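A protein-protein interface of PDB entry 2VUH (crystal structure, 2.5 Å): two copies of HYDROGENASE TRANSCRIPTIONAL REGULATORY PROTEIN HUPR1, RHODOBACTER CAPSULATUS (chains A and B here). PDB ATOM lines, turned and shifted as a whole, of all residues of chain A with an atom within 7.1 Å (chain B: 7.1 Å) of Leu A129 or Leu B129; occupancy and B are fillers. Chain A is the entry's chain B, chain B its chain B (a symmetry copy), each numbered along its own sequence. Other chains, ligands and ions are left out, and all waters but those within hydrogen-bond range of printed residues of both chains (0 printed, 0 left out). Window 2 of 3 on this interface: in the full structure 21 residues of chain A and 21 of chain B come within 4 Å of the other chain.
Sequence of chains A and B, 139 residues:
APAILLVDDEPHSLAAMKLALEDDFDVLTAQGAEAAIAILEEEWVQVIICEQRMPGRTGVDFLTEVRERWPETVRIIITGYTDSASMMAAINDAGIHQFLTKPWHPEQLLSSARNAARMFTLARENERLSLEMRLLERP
O of Asn B126 sits at hydrogen-bond distance from OG of Ser B130 (3.0 Å).
OE2 of Glu B125 is in salt-bridge range of NH1 of Arg B128, at 3.0 Å.
The side-chain hydroxyl of Ser A130 is in hydrogen-bond range of the backbone carbonyl oxygen of Asn A126, at 3.0 Å.
The guanidinium group (NH1) of Arg A128 is in salt-bridge range of the side-chain carboxylate (OE2) of Glu A125 (3.0 Å).
Among the printed residues, merely in contact across the chains: Asn A126 with Leu B129, Leu A129 with Asn B126, Leu A129 with Leu B129, Leu A129 with Ser B130 and Ser A130 with Leu B129.
Glu A125 touches Asn B126, and with the chains exchanged Asn A126 touches Glu B125.
Asn A126 touches Leu B129, and with the chains exchanged Leu A129 touches Asn B126.
Leu B129 touches its own counterpart, Leu A129.
Leu A129 touches Ser B130, and with the chains exchanged Ser A130 touches Leu B129.
Positions printed for both chains: 123, 124, 125, 126, 127, 128, 129, 130, 131, 132, 133, 134 and 135.
Of the 8 pairs that touch across the chains among the printed residues, 8 have their exchanged pair printed and touching as well.
The side-chain carboxylate (OE1) of Glu B125 sits close to the side-chain amide oxygen (OD1) of Asn A126, 3.2 Å away.
ND2 of Asn A126 sits close to ND2 of Asn B126 (2.8 Å).
The side-chain carboxylate of Glu A125 lies close to the side-chain amide oxygen of Asn B126, at 3.2 Å.
Of the 13 printed residues of chain A, 4 touch a printed residue of chain B.
Of the 13 printed residues of chain B, 4 touch a printed residue of chain A.
Printed residues of chain B that touch a printed residue of chain A: Glu B125, Asn B126, Leu B129 and Ser B130.
Hydrophobic or aromatic side chains of chain B that line the printed part of chain A: Leu B129.
Among the printed residues, 8 pairs touch across the chains.
Leu A129 touches just these residues of chain B: Asn B126 (3.4 Å), Leu B129 (3.8 Å) and Ser B130 (3.7 Å).
Printed residues of chain A within 4 Å of Asn B126: Glu A125 (3.2 Å), Asn A126 (2.8 Å) and Leu A129 (3.4 Å).
Of the printed residues of chain B, Asn A126 touches Glu B125 (3.2 Å), Asn B126 (2.8 Å) and Leu B129 (3.4 Å).
Printed residues of chain B within 4 Å of Ser A130: Leu B129 (3.7 Å).
Printed residues of chain A within 4 Å of Ser B130: Leu A129 (3.7 Å).
Printed residues of chain B within 4 Å of Glu A125: Asn B126 (3.2 Å).
Arg A128 touches none of the printed residues of chain B.
Met A133 touches none of the printed residues of chain B.
The nearest residue of chain B that does not touch Leu A129 is Met B133 (5.0 Å).
The nearest residue of chain A that does not touch Leu B129 is Met A133 (5.0 Å).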
ATOM      1  N   ALA A 123      30.841  19.633 -16.659  1.00  0.00           N
ATOM      2  CA  ALA A 123      29.415  19.830 -16.901  1.00  0.00           C
ATOM      3  C   ALA A 123      28.980  19.153 -18.204  1.00  0.00           C
ATOM      4  O   ALA A 123      27.917  18.541 -18.290  1.00  0.00           O
ATOM      5  CB  ALA A 123      29.105  21.314 -16.950  1.00  0.00           C
ATOM      6  N   ARG A 124      29.824  19.268 -19.213  1.00  0.00           N
ATOM      7  CA  ARG A 124      29.482  18.824 -20.539  1.00  0.00           C
ATOM      8  C   ARG A 124      29.504  17.317 -20.551  1.00  0.00           C
ATOM      9  O   ARG A 124      28.628  16.675 -21.116  1.00  0.00           O
ATOM     10  CB  ARG A 124      30.504  19.338 -21.515  1.00  0.00           C
ATOM     11  CG  ARG A 124      29.904  20.018 -22.674  1.00  0.00           C
ATOM     12  CD  ARG A 124      30.980  20.045 -23.740  1.00  0.00           C
ATOM     13  NE  ARG A 124      30.481  19.708 -25.079  1.00  0.00           N
ATOM     14  CZ  ARG A 124      31.257  19.265 -26.071  1.00  0.00           C
ATOM     15  NH1 ARG A 124      32.565  19.096 -25.863  1.00  0.00           N
ATOM     16  NH2 ARG A 124      30.732  18.989 -27.269  1.00  0.00           N
ATOM     17  N   GLU A 125      30.500  16.744 -19.896  1.00  0.00           N
ATOM     18  CA  GLU A 125      30.583  15.302 -19.811  1.00  0.00           C
ATOM     19  C   GLU A 125      29.613  14.728 -18.755  1.00  0.00           C
ATOM     20  O   GLU A 125      29.051  13.659 -18.931  1.00  0.00           O
ATOM     21  CB  GLU A 125      32.040  14.872 -19.625  1.00  0.00           C
ATOM     22  CG  GLU A 125      32.379  13.530 -20.273  1.00  0.00           C
ATOM     23  CD  GLU A 125      32.447  12.437 -19.222  1.00  0.00           C
ATOM     24  OE1 GLU A 125      32.451  12.785 -18.004  1.00  0.00           O
ATOM     25  OE2 GLU A 125      32.504  11.241 -19.594  1.00  0.00           O
ATOM     26  N   ASN A 126      29.368  15.462 -17.691  1.00  0.00           N
ATOM     27  CA  ASN A 126      28.288  15.133 -16.804  1.00  0.00           C
ATOM     28  C   ASN A 126      26.939  14.977 -17.503  1.00  0.00           C
ATOM     29  O   ASN A 126      26.088  14.195 -17.087  1.00  0.00           O
ATOM     30  CB  ASN A 126      28.153  16.252 -15.816  1.00  0.00           C
ATOM     31  CG  ASN A 126      27.648  15.781 -14.507  1.00  0.00           C
ATOM     32  OD1 ASN A 126      26.423  15.846 -14.233  1.00  0.00           O
ATOM     33  ND2 ASN A 126      28.577  15.268 -13.665  1.00  0.00           N
ATOM     34  N   GLU A 127      26.738  15.745 -18.561  1.00  0.00           N
ATOM     35  CA  GLU A 127      25.463  15.792 -19.247  1.00  0.00           C
ATOM     36  C   GLU A 127      25.396  14.659 -20.265  1.00  0.00           C
ATOM     37  O   GLU A 127      24.350  14.048 -20.468  1.00  0.00           O
ATOM     38  CB  GLU A 127      25.298  17.152 -19.914  1.00  0.00           C
ATOM     39  CG  GLU A 127      23.933  17.442 -20.452  1.00  0.00           C
ATOM     40  CD  GLU A 127      24.024  18.092 -21.833  1.00  0.00           C
ATOM     41  OE1 GLU A 127      25.165  18.384 -22.288  1.00  0.00           O
ATOM     42  OE2 GLU A 127      22.960  18.311 -22.469  1.00  0.00           O
ATOM     43  N   ARG A 128      26.537  14.389 -20.884  1.00  0.00           N
ATOM     44  CA  ARG A 128      26.725  13.286 -21.806  1.00  0.00           C
ATOM     45  C   ARG A 128      26.410  11.980 -21.096  1.00  0.00           C
ATOM     46  O   ARG A 128      25.780  11.116 -21.660  1.00  0.00           O
ATOM     47  CB  ARG A 128      28.170  13.291 -22.281  1.00  0.00           C
ATOM     48  CG  ARG A 128      28.449  12.552 -23.559  1.00  0.00           C
ATOM     49  CD  ARG A 128      29.953  12.436 -23.723  1.00  0.00           C
ATOM     50  NE  ARG A 128      30.380  11.064 -24.019  1.00  0.00           N
ATOM     51  CZ  ARG A 128      30.695  10.132 -23.109  1.00  0.00           C
ATOM     52  NH1 ARG A 128      30.642  10.382 -21.797  1.00  0.00           N
ATOM     53  NH2 ARG A 128      31.068   8.933 -23.523  1.00  0.00           N
ATOM     54  N   LEU A 129      26.821  11.841 -19.848  1.00  0.00           N
ATOM     55  CA  LEU A 129      26.531  10.612 -19.119  1.00  0.00           C
ATOM     56  C   LEU A 129      25.037  10.476 -18.768  1.00  0.00           C
ATOM     57  O   LEU A 129      24.521   9.363 -18.810  1.00  0.00           O
ATOM     58  CB  LEU A 129      27.397  10.456 -17.845  1.00  0.00           C
ATOM     59  CG  LEU A 129      28.942  10.499 -17.795  1.00  0.00           C
ATOM     60  CD1 LEU A 129      29.432  10.370 -16.345  1.00  0.00           C
ATOM     61  CD2 LEU A 129      29.646   9.474 -18.708  1.00  0.00           C
ATOM     62  N   SER A 130      24.360  11.582 -18.418  1.00  0.00           N
ATOM     63  CA  SER A 130      22.912  11.580 -18.106  1.00  0.00           C
ATOM     64  C   SER A 130      22.111  11.127 -19.313  1.00  0.00           C
ATOM     65  O   SER A 130      21.312  10.195 -19.222  1.00  0.00           O
ATOM     66  CB  SER A 130      22.431  12.959 -17.687  1.00  0.00           C
ATOM     67  OG  SER A 130      23.241  13.458 -16.653  1.00  0.00           O
ATOM     68  N   LEU A 131      22.358  11.796 -20.440  1.00  0.00           N
ATOM     69  CA  LEU A 131      21.733  11.483 -21.713  1.00  0.00           C
ATOM     70  C   LEU A 131      22.003  10.045 -22.092  1.00  0.00           C
ATOM     71  O   LEU A 131      21.099   9.334 -22.496  1.00  0.00           O
ATOM     72  CB  LEU A 131      22.197  12.425 -22.838  1.00  0.00           C
ATOM     73  CG  LEU A 131      22.043  13.959 -22.740  1.00  0.00           C
ATOM     74  CD1 LEU A 131      22.183  14.611 -24.119  1.00  0.00           C
ATOM     75  CD2 LEU A 131      20.755  14.445 -22.001  1.00  0.00           C
ATOM     76  N   GLU A 132      23.230   9.586 -21.942  1.00  0.00           N
ATOM     77  CA  GLU A 132      23.518   8.241 -22.402  1.00  0.00           C
ATOM     78  C   GLU A 132      22.978   7.157 -21.508  1.00  0.00           C
ATOM     79  O   GLU A 132      22.557   6.129 -22.011  1.00  0.00           O
ATOM     80  CB  GLU A 132      24.993   8.045 -22.746  1.00  0.00           C
ATOM     81  CG  GLU A 132      25.278   8.640 -24.115  1.00  0.00           C
ATOM     82  CD  GLU A 132      26.560   8.163 -24.733  1.00  0.00           C
ATOM     83  OE1 GLU A 132      27.644   8.478 -24.184  1.00  0.00           O
ATOM     84  OE2 GLU A 132      26.474   7.496 -25.794  1.00  0.00           O
ATOM     85  N   MET A 133      22.951   7.395 -20.204  1.00  0.00           N
ATOM     86  CA  MET A 133      22.441   6.397 -19.287  1.00  0.00           C
ATOM     87  C   MET A 133      20.917   6.234 -19.455  1.00  0.00           C
ATOM     88  O   MET A 133      20.406   5.088 -19.497  1.00  0.00           O
ATOM     89  CB  MET A 133      22.855   6.708 -17.850  1.00  0.00           C
ATOM     90  CG  MET A 133      21.773   6.457 -16.814  1.00  0.00           C
ATOM     91  SD  MET A 133      22.419   5.921 -15.214  1.00  0.00           S
ATOM     92  CE  MET A 133      20.894   5.457 -14.338  1.00  0.00           C
ATOM     93  N   ARG A 134      20.204   7.364 -19.576  1.00  0.00           N
ATOM     94  CA  ARG A 134      18.774   7.358 -19.902  1.00  0.00           C
ATOM     95  C   ARG A 134      18.454   6.350 -20.999  1.00  0.00           C
ATOM     96  O   ARG A 134      17.499   5.580 -20.868  1.00  0.00           O
ATOM     97  CB  ARG A 134      18.319   8.722 -20.374  1.00  0.00           C
ATOM     98  CG  ARG A 134      17.640   9.519 -19.324  1.00  0.00           C
ATOM     99  CD  ARG A 134      17.026  10.732 -19.972  1.00  0.00           C
ATOM    100  NE  ARG A 134      17.063  11.863 -19.060  1.00  0.00           N
ATOM    101  CZ  ARG A 134      17.430  13.098 -19.394  1.00  0.00           C
ATOM    102  NH1 ARG A 134      17.807  13.384 -20.634  1.00  0.00           N
ATOM    103  NH2 ARG A 134      17.434  14.055 -18.472  1.00  0.00           N
ATOM    104  N   LEU A 135      19.255   6.363 -22.068  1.00  0.00           N
ATOM    105  CA  LEU A 135      19.172   5.379 -23.150  1.00  0.00           C
ATOM    106  C   LEU A 135      19.744   3.986 -22.769  1.00  0.00           C
ATOM    107  O   LEU A 135      19.366   3.369 -21.754  1.00  0.00           O
ATOM    108  CB  LEU A 135      19.880   5.932 -24.401  1.00  0.00           C
ATOM    109  CG  LEU A 135      19.578   7.355 -24.908  1.00  0.00           C
ATOM    110  CD1 LEU A 135      20.613   7.856 -25.924  1.00  0.00           C
ATOM    111  CD2 LEU A 135      18.187   7.451 -25.509  1.00  0.00           C
ATOM    112  N   ALA B 123      32.328  16.835 -10.049  1.00  0.00           N
ATOM    113  CA  ALA B 123      33.236  15.691 -10.090  1.00  0.00           C
ATOM    114  C   ALA B 123      32.639  14.491  -9.351  1.00  0.00           C
ATOM    115  O   ALA B 123      32.740  13.347  -9.791  1.00  0.00           O
ATOM    116  CB  ALA B 123      34.570  16.076  -9.481  1.00  0.00           C
ATOM    117  N   ARG B 124      32.014  14.772  -8.223  1.00  0.00           N
ATOM    118  CA  ARG B 124      31.543  13.735  -7.340  1.00  0.00           C
ATOM    119  C   ARG B 124      30.339  13.088  -7.975  1.00  0.00           C
ATOM    120  O   ARG B 124      30.196  11.873  -7.966  1.00  0.00           O
ATOM    121  CB  ARG B 124      31.139  14.347  -6.027  1.00  0.00           C
ATOM    122  CG  ARG B 124      31.742  13.671  -4.867  1.00  0.00           C
ATOM    123  CD  ARG B 124      30.900  14.073  -3.672  1.00  0.00           C
ATOM    124  NE  ARG B 124      30.601  12.955  -2.769  1.00  0.00           N
ATOM    125  CZ  ARG B 124      29.577  12.946  -1.913  1.00  0.00           C
ATOM    126  NH1 ARG B 124      28.751  13.993  -1.858  1.00  0.00           N
ATOM    127  NH2 ARG B 124      29.372  11.894  -1.113  1.00  0.00           N
ATOM    128  N   GLU B 125      29.478  13.906  -8.556  1.00  0.00           N
ATOM    129  CA  GLU B 125      28.312  13.376  -9.232  1.00  0.00           C
ATOM    130  C   GLU B 125      28.660  12.814 -10.628  1.00  0.00           C
ATOM    131  O   GLU B 125      28.092  11.828 -11.069  1.00  0.00           O
ATOM    132  CB  GLU B 125      27.191  14.418  -9.234  1.00  0.00           C
ATOM    133  CG  GLU B 125      25.787  13.818  -9.169  1.00  0.00           C
ATOM    134  CD  GLU B 125      25.134  13.847 -10.539  1.00  0.00           C
ATOM    135  OE1 GLU B 125      25.695  14.527 -11.448  1.00  0.00           O
ATOM    136  OE2 GLU B 125      24.071  13.208 -10.717  1.00  0.00           O
ATOM    137  N   ASN B 126      29.629  13.402 -11.296  1.00  0.00           N
ATOM    138  CA  ASN B 126      30.192  12.788 -12.466  1.00  0.00           C
ATOM    139  C   ASN B 126      30.668  11.354 -12.244  1.00  0.00           C
ATOM    140  O   ASN B 126      30.633  10.519 -13.144  1.00  0.00           O
ATOM    141  CB  ASN B 126      31.384  13.597 -12.876  1.00  0.00           C
ATOM    142  CG  ASN B 126      31.609  13.556 -14.338  1.00  0.00           C
ATOM    143  OD1 ASN B 126      32.420  12.736 -14.839  1.00  0.00           O
ATOM    144  ND2 ASN B 126      30.876  14.427 -15.073  1.00  0.00           N
ATOM    145  N   GLU B 127      31.138  11.076 -11.039  1.00  0.00           N
ATOM    146  CA  GLU B 127      31.736   9.795 -10.723  1.00  0.00           C
ATOM    147  C   GLU B 127      30.640   8.807 -10.340  1.00  0.00           C
ATOM    148  O   GLU B 127      30.702   7.627 -10.674  1.00  0.00           O
ATOM    149  CB  GLU B 127      32.745   9.972  -9.595  1.00  0.00           C
ATOM    150  CG  GLU B 127      33.620   8.790  -9.325  1.00  0.00           C
ATOM    151  CD  GLU B 127      33.755   8.552  -7.820  1.00  0.00           C
ATOM    152  OE1 GLU B 127      33.230   9.383  -7.028  1.00  0.00           O
ATOM    153  OE2 GLU B 127      34.380   7.533  -7.423  1.00  0.00           O
ATOM    154  N   ARG B 128      29.632   9.322  -9.648  1.00  0.00           N
ATOM    155  CA  ARG B 128      28.438   8.590  -9.276  1.00  0.00           C
ATOM    156  C   ARG B 128      27.754   8.076 -10.532  1.00  0.00           C
ATOM    157  O   ARG B 128      27.296   6.957 -10.562  1.00  0.00           O
ATOM    158  CB  ARG B 128      27.509   9.527  -8.518  1.00  0.00           C
ATOM    159  CG  ARG B 128      26.466   8.873  -7.659  1.00  0.00           C
ATOM    160  CD  ARG B 128      25.483   9.938  -7.210  1.00  0.00           C
ATOM    161  NE  ARG B 128      24.088   9.547  -7.442  1.00  0.00           N
ATOM    162  CZ  ARG B 128      23.390   9.780  -8.562  1.00  0.00           C
ATOM    163  NH1 ARG B 128      23.928  10.413  -9.609  1.00  0.00           N
ATOM    164  NH2 ARG B 128      22.135   9.370  -8.630  1.00  0.00           N
ATOM    165  N   LEU B 129      27.706   8.877 -11.582  1.00  0.00           N
ATOM    166  CA  LEU B 129      27.074   8.424 -12.814  1.00  0.00           C
ATOM    167  C   LEU B 129      27.897   7.337 -13.532  1.00  0.00           C
ATOM    168  O   LEU B 129      27.301   6.424 -14.097  1.00  0.00           O
ATOM    169  CB  LEU B 129      26.761   9.588 -13.787  1.00  0.00           C
ATOM    170  CG  LEU B 129      25.930  10.848 -13.446  1.00  0.00           C
ATOM    171  CD1 LEU B 129      25.894  11.804 -14.648  1.00  0.00           C
ATOM    172  CD2 LEU B 129      24.507  10.562 -12.926  1.00  0.00           C
ATOM    173  N   SER B 130      29.235   7.439 -13.520  1.00  0.00           N
ATOM    174  CA  SER B 130      30.129   6.430 -14.135  1.00  0.00           C
ATOM    175  C   SER B 130      29.940   5.078 -13.469  1.00  0.00           C
ATOM    176  O   SER B 130      29.679   4.079 -14.139  1.00  0.00           O
ATOM    177  CB  SER B 130      31.589   6.835 -14.019  1.00  0.00           C
ATOM    178  OG  SER B 130      31.768   8.138 -14.513  1.00  0.00           O
ATOM    179  N   LEU B 131      30.061   5.081 -12.140  1.00  0.00           N
ATOM    180  CA  LEU B 131      29.867   3.902 -11.315  1.00  0.00           C
ATOM    181  C   LEU B 131      28.491   3.322 -11.541  1.00  0.00           C
ATOM    182  O   LEU B 131      28.346   2.124 -11.709  1.00  0.00           O
ATOM    183  CB  LEU B 131      30.082   4.195  -9.820  1.00  0.00           C
ATOM    184  CG  LEU B 131      31.402   4.788  -9.280  1.00  0.00           C
ATOM    185  CD1 LEU B 131      31.512   4.590  -7.765  1.00  0.00           C
ATOM    186  CD2 LEU B 131      32.692   4.303 -10.019  1.00  0.00           C
ATOM    187  N   GLU B 132      27.468   4.153 -11.580  1.00  0.00           N
ATOM    188  CA  GLU B 132      26.135   3.594 -11.690  1.00  0.00           C
ATOM    189  C   GLU B 132      25.797   3.079 -13.064  1.00  0.00           C
ATOM    190  O   GLU B 132      25.106   2.080 -13.168  1.00  0.00           O
ATOM    191  CB  GLU B 132      25.062   4.524 -11.126  1.00  0.00           C
ATOM    192  CG  GLU B 132      25.046   4.419  -9.610  1.00  0.00           C
ATOM    193  CD  GLU B 132      23.797   4.955  -8.975  1.00  0.00           C
ATOM    194  OE1 GLU B 132      23.561   6.186  -9.060  1.00  0.00           O
ATOM    195  OE2 GLU B 132      23.069   4.138  -8.359  1.00  0.00           O
ATOM    196  N   MET B 133      26.308   3.723 -14.103  1.00  0.00           N
ATOM    197  CA  MET B 133      26.028   3.279 -15.452  1.00  0.00           C
ATOM    198  C   MET B 133      26.723   1.934 -15.736  1.00  0.00           C
ATOM    199  O   MET B 133      26.099   1.010 -16.316  1.00  0.00           O
ATOM    200  CB  MET B 133      26.378   4.362 -16.471  1.00  0.00           C
ATOM    201  CG  MET B 133      27.039   3.845 -17.738  1.00  0.00           C
ATOM    202  SD  MET B 133      26.627   4.809 -19.210  1.00  0.00           S
ATOM    203  CE  MET B 133      27.333   3.780 -20.533  1.00  0.00           C
ATOM    204  N   ARG B 134      27.990   1.814 -15.313  1.00  0.00           N
ATOM    205  CA  ARG B 134      28.720   0.542 -15.370  1.00  0.00           C
ATOM    206  C   ARG B 134      27.845  -0.625 -14.924  1.00  0.00           C
ATOM    207  O   ARG B 134      27.811  -1.658 -15.597  1.00  0.00           O
ATOM    208  CB  ARG B 134      29.942   0.576 -14.479  1.00  0.00           C
ATOM    209  CG  ARG B 134      31.205   0.842 -15.210  1.00  0.00           C
ATOM    210  CD  ARG B 134      32.356   0.610 -14.268  1.00  0.00           C
ATOM    211  NE  ARG B 134      33.444   1.527 -14.567  1.00  0.00           N
ATOM    212  CZ  ARG B 134      34.131   2.213 -13.656  1.00  0.00           C
ATOM    213  NH1 ARG B 134      33.849   2.102 -12.364  1.00  0.00           N
ATOM    214  NH2 ARG B 134      35.102   3.033 -14.045  1.00  0.00           N
ATOM    215  N   LEU B 135      27.149  -0.447 -13.799  1.00  0.00           N
ATOM    216  CA  LEU B 135      26.164  -1.410 -13.300  1.00  0.00           C
ATOM    217  C   LEU B 135      24.831  -1.406 -14.098  1.00  0.00           C
ATOM    218  O   LEU B 135      24.798  -1.537 -15.337  1.00  0.00           O
ATOM    219  CB  LEU B 135      25.903  -1.149 -11.806  1.00  0.00           C
ATOM    220  CG  LEU B 135      27.077  -0.983 -10.822  1.00  0.00           C
ATOM    221  CD1 LEU B 135      26.644  -0.385  -9.476  1.00  0.00           C
ATOM    222  CD2 LEU B 135      27.800  -2.297 -10.586  1.00  0.00           C
